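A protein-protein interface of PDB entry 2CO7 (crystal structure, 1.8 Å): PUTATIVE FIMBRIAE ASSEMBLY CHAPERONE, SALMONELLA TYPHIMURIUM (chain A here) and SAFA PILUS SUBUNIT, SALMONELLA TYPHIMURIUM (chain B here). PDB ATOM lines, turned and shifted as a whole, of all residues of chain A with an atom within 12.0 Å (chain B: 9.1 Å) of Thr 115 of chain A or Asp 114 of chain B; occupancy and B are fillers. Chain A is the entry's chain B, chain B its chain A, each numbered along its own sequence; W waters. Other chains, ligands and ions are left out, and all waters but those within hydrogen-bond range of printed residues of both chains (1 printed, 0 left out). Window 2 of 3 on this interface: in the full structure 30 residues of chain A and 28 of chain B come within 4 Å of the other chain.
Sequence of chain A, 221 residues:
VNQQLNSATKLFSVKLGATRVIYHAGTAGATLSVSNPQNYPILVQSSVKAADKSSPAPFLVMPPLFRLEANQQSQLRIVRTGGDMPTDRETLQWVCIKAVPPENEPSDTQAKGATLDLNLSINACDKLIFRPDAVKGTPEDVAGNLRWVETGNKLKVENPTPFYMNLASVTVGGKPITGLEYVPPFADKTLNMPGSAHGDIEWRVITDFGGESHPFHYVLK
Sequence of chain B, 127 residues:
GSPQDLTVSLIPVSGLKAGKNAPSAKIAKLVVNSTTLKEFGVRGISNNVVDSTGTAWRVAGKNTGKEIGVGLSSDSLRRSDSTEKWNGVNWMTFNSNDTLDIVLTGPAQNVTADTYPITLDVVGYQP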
ATOM      1  N   ALA A   8       2.278  -2.691 -10.699  1.00  0.00           N
ATOM      2  CA  ALA A   8       2.904  -3.577  -9.680  1.00  0.00           C
ATOM      3  C   ALA A   8       3.760  -2.819  -8.662  1.00  0.00           C
ATOM      4  O   ALA A   8       4.555  -3.442  -7.958  1.00  0.00           O
ATOM      5  CB  ALA A   8       3.719  -4.675 -10.352  1.00  0.00           C
ATOM      6  N   THR A   9       3.616  -1.493  -8.577  1.00  0.00           N
ATOM      7  CA  THR A   9       4.215  -0.751  -7.447  1.00  0.00           C
ATOM      8  C   THR A   9       3.402  -1.050  -6.181  1.00  0.00           C
ATOM      9  O   THR A   9       2.169  -0.977  -6.203  1.00  0.00           O
ATOM     10  CB  THR A   9       4.291   0.798  -7.676  1.00  0.00           C
ATOM     11  OG1 THR A   9       5.261   1.106  -8.685  1.00  0.00           O
ATOM     12  CG2 THR A   9       4.713   1.517  -6.408  1.00  0.00           C
ATOM     13  N   LYS A  10       4.092  -1.387  -5.090  1.00  0.00           N
ATOM     14  CA  LYS A  10       3.455  -1.523  -3.788  1.00  0.00           C
ATOM     15  C   LYS A  10       3.602  -0.226  -3.015  1.00  0.00           C
ATOM     16  O   LYS A  10       4.721   0.254  -2.787  1.00  0.00           O
ATOM     17  CB  LYS A  10       4.075  -2.659  -2.965  1.00  0.00           C
ATOM     18  CG  LYS A  10       3.463  -2.822  -1.552  1.00  0.00           C
ATOM     19  CD  LYS A  10       1.971  -3.187  -1.606  1.00  0.00           C
ATOM     20  CE  LYS A  10       1.249  -3.051  -0.246  1.00  0.00           C
ATOM     21  NZ  LYS A  10       0.089  -4.042  -0.170  1.00  0.00           N
ATOM     22  N   THR A 115       9.204 -12.184 -12.436  1.00  0.00           N
ATOM     23  CA  THR A 115       8.418 -11.108 -11.835  1.00  0.00           C
ATOM     24  C   THR A 115       8.586 -11.091 -10.321  1.00  0.00           C
ATOM     25  O   THR A 115       9.061 -12.067  -9.725  1.00  0.00           O
ATOM     26  CB  THR A 115       6.907 -11.232 -12.163  1.00  0.00           C
ATOM     27  OG1 THR A 115       6.389 -12.456 -11.620  1.00  0.00           O
ATOM     28  CG2 THR A 115       6.673 -11.203 -13.673  1.00  0.00           C
ATOM     29  N   LEU A 116       8.191  -9.980  -9.702  1.00  0.00           N
ATOM     30  CA  LEU A 116       8.294  -9.864  -8.249  1.00  0.00           C
ATOM     31  C   LEU A 116       6.927  -9.744  -7.565  1.00  0.00           C
ATOM     32  O   LEU A 116       5.962  -9.207  -8.136  1.00  0.00           O
ATOM     33  CB  LEU A 116       9.226  -8.705  -7.847  1.00  0.00           C
ATOM     34  CG  LEU A 116      10.711  -8.715  -8.259  1.00  0.00           C
ATOM     35  CD1 LEU A 116      11.466  -7.542  -7.617  1.00  0.00           C
ATOM     36  CD2 LEU A 116      11.419 -10.035  -7.931  1.00  0.00           C
ATOM     37  N   ASP A 117       6.855 -10.292  -6.356  1.00  0.00           N
ATOM     38  CA  ASP A 117       5.716 -10.106  -5.461  1.00  0.00           C
ATOM     39  C   ASP A 117       6.202  -9.231  -4.299  1.00  0.00           C
ATOM     40  O   ASP A 117       6.848  -9.702  -3.353  1.00  0.00           O
ATOM     41  CB  ASP A 117       5.174 -11.463  -4.985  1.00  0.00           C
ATOM     42  CG  ASP A 117       4.084 -11.342  -3.907  1.00  0.00           C
ATOM     43  OD1 ASP A 117       3.237 -10.412  -3.959  1.00  0.00           O
ATOM     44  OD2 ASP A 117       4.090 -12.201  -2.992  1.00  0.00           O
ATOM     45  N   LEU A 118       5.877  -7.949  -4.409  1.00  0.00           N
ATOM     46  CA  LEU A 118       6.389  -6.902  -3.535  1.00  0.00           C
ATOM     47  C   LEU A 118       5.438  -6.641  -2.378  1.00  0.00           C
ATOM     48  O   LEU A 118       4.243  -6.424  -2.587  1.00  0.00           O
ATOM     49  CB  LEU A 118       6.536  -5.619  -4.351  1.00  0.00           C
ATOM     50  CG  LEU A 118       7.804  -5.317  -5.179  1.00  0.00           C
ATOM     51  CD1 LEU A 118       8.765  -6.458  -5.346  1.00  0.00           C
ATOM     52  CD2 LEU A 118       7.453  -4.691  -6.477  1.00  0.00           C
ATOM     53  N   ASN A 119       5.950  -6.641  -1.156  1.00  0.00           N
ATOM     54  CA  ASN A 119       5.101  -6.200  -0.034  1.00  0.00           C
ATOM     55  C   ASN A 119       5.903  -5.448   1.008  1.00  0.00           C
ATOM     56  O   ASN A 119       7.139  -5.459   0.998  1.00  0.00           O
ATOM     57  CB  ASN A 119       4.305  -7.366   0.589  1.00  0.00           C
ATOM     58  CG  ASN A 119       2.851  -6.965   1.005  1.00  0.00           C
ATOM     59  OD1 ASN A 119       1.995  -7.836   1.288  1.00  0.00           O
ATOM     60  ND2 ASN A 119       2.563  -5.667   1.004  1.00  0.00           N
ATOM     61  N   PRO B  12       8.896  -1.987  -8.878  1.00  0.00           N
ATOM     62  CA  PRO B  12       9.651  -2.972  -9.659  1.00  0.00           C
ATOM     63  C   PRO B  12      10.449  -2.261 -10.742  1.00  0.00           C
ATOM     64  O   PRO B  12       9.989  -1.230 -11.246  1.00  0.00           O
ATOM     65  CB  PRO B  12       8.552  -3.826 -10.302  1.00  0.00           C
ATOM     66  CG  PRO B  12       7.373  -2.929 -10.368  1.00  0.00           C
ATOM     67  CD  PRO B  12       7.444  -2.116  -9.107  1.00  0.00           C
ATOM     68  N   VAL B  13      11.626  -2.797 -11.065  1.00  0.00           N
ATOM     69  CA  VAL B  13      12.518  -2.222 -12.075  1.00  0.00           C
ATOM     70  C   VAL B  13      12.554  -3.102 -13.334  1.00  0.00           C
ATOM     71  O   VAL B  13      12.527  -4.333 -13.247  1.00  0.00           O
ATOM     72  CB  VAL B  13      13.962  -2.021 -11.526  1.00  0.00           C
ATOM     73  CG1 VAL B  13      14.947  -1.709 -12.666  1.00  0.00           C
ATOM     74  CG2 VAL B  13      13.997  -0.932 -10.458  1.00  0.00           C
ATOM     75  N   ASN B  21      21.187 -13.163 -15.335  1.00  0.00           N
ATOM     76  CA  ASN B  21      21.052 -11.710 -15.167  1.00  0.00           C
ATOM     77  C   ASN B  21      22.389 -10.982 -15.059  1.00  0.00           C
ATOM     78  O   ASN B  21      23.417 -11.592 -14.745  1.00  0.00           O
ATOM     79  CB  ASN B  21      20.167 -11.370 -13.950  1.00  0.00           C
ATOM     80  CG  ASN B  21      18.748 -11.863 -14.121  1.00  0.00           C
ATOM     81  OD1 ASN B  21      17.815 -10.968 -14.927  1.00  0.00           O
ATOM     82  ND2 ASN B  21      18.623 -13.162 -13.747  1.00  0.00           N
ATOM     83  N   ILE B  27      16.497  -4.638  -9.367  1.00  0.00           N
ATOM     84  CA  ILE B  27      15.221  -5.363  -9.448  1.00  0.00           C
ATOM     85  C   ILE B  27      14.039  -4.605  -8.818  1.00  0.00           C
ATOM     86  O   ILE B  27      12.887  -4.829  -9.196  1.00  0.00           O
ATOM     87  CB  ILE B  27      15.312  -6.822  -8.879  1.00  0.00           C
ATOM     88  CG1 ILE B  27      15.858  -6.844  -7.445  1.00  0.00           C
ATOM     89  CG2 ILE B  27      16.175  -7.691  -9.787  1.00  0.00           C
ATOM     90  CD1 ILE B  27      15.388  -8.055  -6.625  1.00  0.00           C
ATOM     91  N   VAL B  59      15.835 -15.198  -1.434  1.00  0.00           N
ATOM     92  CA  VAL B  59      14.412 -15.154  -1.745  1.00  0.00           C
ATOM     93  C   VAL B  59      13.974 -16.358  -2.625  1.00  0.00           C
ATOM     94  O   VAL B  59      14.575 -16.623  -3.681  1.00  0.00           O
ATOM     95  CB  VAL B  59      14.068 -13.777  -2.365  1.00  0.00           C
ATOM     96  CG1 VAL B  59      12.957 -13.866  -3.389  1.00  0.00           C
ATOM     97  CG2 VAL B  59      13.740 -12.753  -1.253  1.00  0.00           C
ATOM     98  N   ALA B  60      12.933 -17.068  -2.166  1.00  0.00           N
ATOM     99  CA  ALA B  60      12.477 -18.338  -2.760  1.00  0.00           C
ATOM    100  C   ALA B  60      11.269 -18.156  -3.685  1.00  0.00           C
ATOM    101  O   ALA B  60      10.207 -17.698  -3.254  1.00  0.00           O
ATOM    102  CB  ALA B  60      12.151 -19.335  -1.660  1.00  0.00           C
ATOM    103  N   GLY B  61      11.435 -18.532  -4.950  1.00  0.00           N
ATOM    104  CA  GLY B  61      10.418 -18.302  -5.984  1.00  0.00           C
ATOM    105  C   GLY B  61       9.033 -18.835  -5.671  1.00  0.00           C
ATOM    106  O   GLY B  61       8.859 -20.033  -5.459  1.00  0.00           O
ATOM    107  N   ILE B  68      17.072 -16.895  -5.115  1.00  0.00           N
ATOM    108  CA  ILE B  68      17.953 -15.824  -5.591  1.00  0.00           C
ATOM    109  C   ILE B  68      18.435 -14.928  -4.453  1.00  0.00           C
ATOM    110  O   ILE B  68      17.717 -14.705  -3.471  1.00  0.00           O
ATOM    111  CB  ILE B  68      17.276 -14.974  -6.697  1.00  0.00           C
ATOM    112  CG1 ILE B  68      15.956 -14.376  -6.176  1.00  0.00           C
ATOM    113  CG2 ILE B  68      17.091 -15.817  -7.977  1.00  0.00           C
ATOM    114  CD1 ILE B  68      15.394 -13.256  -7.010  1.00  0.00           C
ATOM    115  N   THR B 112      15.349 -18.430 -12.989  1.00  0.00           N
ATOM    116  CA  THR B 112      14.205 -19.343 -13.072  1.00  0.00           C
ATOM    117  C   THR B 112      12.883 -18.585 -13.280  1.00  0.00           C
ATOM    118  O   THR B 112      12.524 -17.693 -12.486  1.00  0.00           O
ATOM    119  CB  THR B 112      14.143 -20.287 -11.836  1.00  0.00           C
ATOM    120  OG1 THR B 112      15.138 -21.320 -11.976  1.00  0.00           O
ATOM    121  CG2 THR B 112      12.754 -20.948 -11.696  1.00  0.00           C
ATOM    122  N   ALA B 113      12.177 -18.946 -14.358  1.00  0.00           N
ATOM    123  CA  ALA B 113      10.861 -18.381 -14.679  1.00  0.00           C
ATOM    124  C   ALA B 113       9.890 -18.658 -13.541  1.00  0.00           C
ATOM    125  O   ALA B 113       9.398 -19.782 -13.381  1.00  0.00           O
ATOM    126  CB  ALA B 113      10.326 -18.953 -15.991  1.00  0.00           C
ATOM    127  N   ASP B 114       9.637 -17.620 -12.744  1.00  0.00           N
ATOM    128  CA  ASP B 114       8.866 -17.745 -11.514  1.00  0.00           C
ATOM    129  C   ASP B 114       8.470 -16.350 -10.999  1.00  0.00           C
ATOM    130  O   ASP B 114       8.889 -15.326 -11.565  1.00  0.00           O
ATOM    131  CB  ASP B 114       9.706 -18.493 -10.457  1.00  0.00           C
ATOM    132  CG  ASP B 114       8.849 -19.240  -9.425  1.00  0.00           C
ATOM    133  OD1 ASP B 114       9.430 -19.954  -8.573  1.00  0.00           O
ATOM    134  OD2 ASP B 114       7.601 -19.125  -9.461  1.00  0.00           O
ATOM    135  N   THR B 115       7.633 -16.327  -9.957  1.00  0.00           N
ATOM    136  CA  THR B 115       7.310 -15.114  -9.176  1.00  0.00           C
ATOM    137  C   THR B 115       8.091 -15.180  -7.860  1.00  0.00           C
ATOM    138  O   THR B 115       8.016 -16.191  -7.157  1.00  0.00           O
ATOM    139  CB  THR B 115       5.793 -15.047  -8.820  1.00  0.00           C
ATOM    140  OG1 THR B 115       4.988 -15.389  -9.958  1.00  0.00           O
ATOM    141  CG2 THR B 115       5.391 -13.654  -8.304  1.00  0.00           C
ATOM    142  N   TYR B 116       8.830 -14.114  -7.525  1.00  0.00           N
ATOM    143  CA  TYR B 116       9.643 -14.082  -6.295  1.00  0.00           C
ATOM    144  C   TYR B 116       9.158 -13.029  -5.293  1.00  0.00           C
ATOM    145  O   TYR B 116       8.912 -11.871  -5.664  1.00  0.00           O
ATOM    146  CB  TYR B 116      11.127 -13.850  -6.615  1.00  0.00           C
ATOM    147  CG  TYR B 116      11.838 -15.013  -7.279  1.00  0.00           C
ATOM    148  CD1 TYR B 116      11.598 -15.331  -8.613  1.00  0.00           C
ATOM    149  CD2 TYR B 116      12.774 -15.778  -6.578  1.00  0.00           C
ATOM    150  CE1 TYR B 116      12.249 -16.390  -9.228  1.00  0.00           C
ATOM    151  CE2 TYR B 116      13.441 -16.847  -7.193  1.00  0.00           C
ATOM    152  CZ  TYR B 116      13.168 -17.145  -8.516  1.00  0.00           C
ATOM    153  OH  TYR B 116      13.818 -18.187  -9.150  1.00  0.00           O
ATOM    154  N   PRO B 117       9.028 -13.423  -4.008  1.00  0.00           N
ATOM    155  CA  PRO B 117       8.485 -12.527  -2.992  1.00  0.00           C
ATOM    156  C   PRO B 117       9.578 -11.676  -2.346  1.00  0.00           C
ATOM    157  O   PRO B 117      10.577 -12.202  -1.847  1.00  0.00           O
ATOM    158  CB  PRO B 117       7.881 -13.492  -1.972  1.00  0.00           C
ATOM    159  CG  PRO B 117       8.775 -14.714  -2.062  1.00  0.00           C
ATOM    160  CD  PRO B 117       9.397 -14.731  -3.435  1.00  0.00           C
ATOM    161  N   ILE B 118       9.390 -10.363  -2.362  1.00  0.00           N
ATOM    162  CA  ILE B 118      10.330  -9.485  -1.699  1.00  0.00           C
ATOM    163  C   ILE B 118       9.579  -8.674  -0.657  1.00  0.00           C
ATOM    164  O   ILE B 118       8.617  -7.972  -0.976  1.00  0.00           O
ATOM    165  CB  ILE B 118      11.043  -8.535  -2.679  1.00  0.00           C
ATOM    166  CG1 ILE B 118      11.831  -9.315  -3.752  1.00  0.00           C
ATOM    167  CG2 ILE B 118      11.921  -7.551  -1.912  1.00  0.00           C
ATOM    168  CD1 ILE B 118      13.243  -9.718  -3.348  1.00  0.00           C
HETATM  169  O   HOH W   1       6.051 -10.037  -0.908  1.00  0.00           O
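N of Tyr 116 of chain B lies within hydrogen-bond range of O of Thr 115 of chain A (3.0 Å). N of Asn 119 of chain A is in hydrogen-bond range of O of Ile 118 of chain B (3.0 Å). The backbone carbonyl oxygen of Asp 114 of chain B is in hydrogen-bond range of the backbone NH of Thr 115 of chain A, 3.3 Å away. O of Tyr 116 of chain B is in hydrogen-bond range of N of Asp 117 of chain A (2.7 Å). O of Asp 117 of chain A lies within hydrogen-bond range of N of Ile 118 of chain B, at 2.8 Å.
N of Val 13 of chain B sits at hydrogen-bond distance from O of Ile 27 of chain B, at 3.0 Å. The side-chain amino group (NZ) of Lys 10 of chain A lies close to the side-chain amide nitrogen (ND2) of Asn 119 of chain A (3.2 Å).
Pro 12 of chain B touches Ala 8 of chain A (CD to O, 3.4 Å). CA of Thr 9 of chain A touches CD of Pro 12 of chain B (3.9 Å). O of Thr 115 of chain A touches CA of Thr 115 of chain B (3.6 Å). Leu 116 of chain A touches Ile 27 of chain B. O of Tyr 116 of chain B touches CA of Leu 116 of chain A (3.3 Å). Asp 117 of chain A touches Thr 115 of chain B. Asp 117 of chain A touches Pro 117 of chain B. Pro 12 of chain B touches Leu 118 of chain A (CD to CD2, 3.7 Å). Ile 118 of chain B touches Leu 118 of chain A (O to CA, 3.6 Å).
Printed residues of chain B within 4 Å of Thr 9 of chain A: Pro 12 (3.9 Å). Printed residues of chain B within 4 Å of Asn 119 of chain A: Ile 118 (3.0 Å). Printed residues of chain A within 4 Å of Pro 12 of chain B: Ala 8, Thr 9 and Leu 118. Printed residues of chain A within 4 Å of Ile 27 of chain B: Leu 116. Ala 60 of chain B touches none of the printed residues of chain A. No residue of chain A comes within 4 Å of Gly 61 of chain B. Ile 68 of chain B touches none of the printed residues of chain A. No residue of chain A comes within 4 Å of Thr 112 of chain B. No residue of chain A comes within 4 Å of Ala 113 of chain B. Of chain A, only Thr 115 comes within 4 Å of Asp 114 of chain B. Printed residues of chain A within 4 Å of Thr 115 of chain B: Thr 115 (3.6 Å) and Asp 117 (3.98 Å). Tyr 116 of chain B touches just these residues of chain A: Thr 115, Leu 116 and Asp 117. The nearest residue of chain B that does not touch Thr 115 of chain A is Pro 117 of chain B (5.9 Å). The nearest residue of chain A that does not touch Asp 114 of chain B is Leu 116 of chain A (5.7 Å). The nearest printed residue of chain B that does not touch Leu 116 of chain A is Ile 118 of chain B (4.3 Å).
Of the 8 printed residues of chain A, 7 touch a printed residue of chain B. Printed residues of chain A that touch a printed residue of chain B: Ala 8, Thr 9, Thr 115, Leu 116, Asp 117, Leu 118 and Asn 119. Hydrophobic or aromatic side chains of chain A within 4 Å of the printed part of chain B: Leu 116 and Leu 118.
Water W1 lies within hydrogen-bond range of O of Asp 117 of chain A, O of Ile 118 of chain B and N of Asn 119 of chain A.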
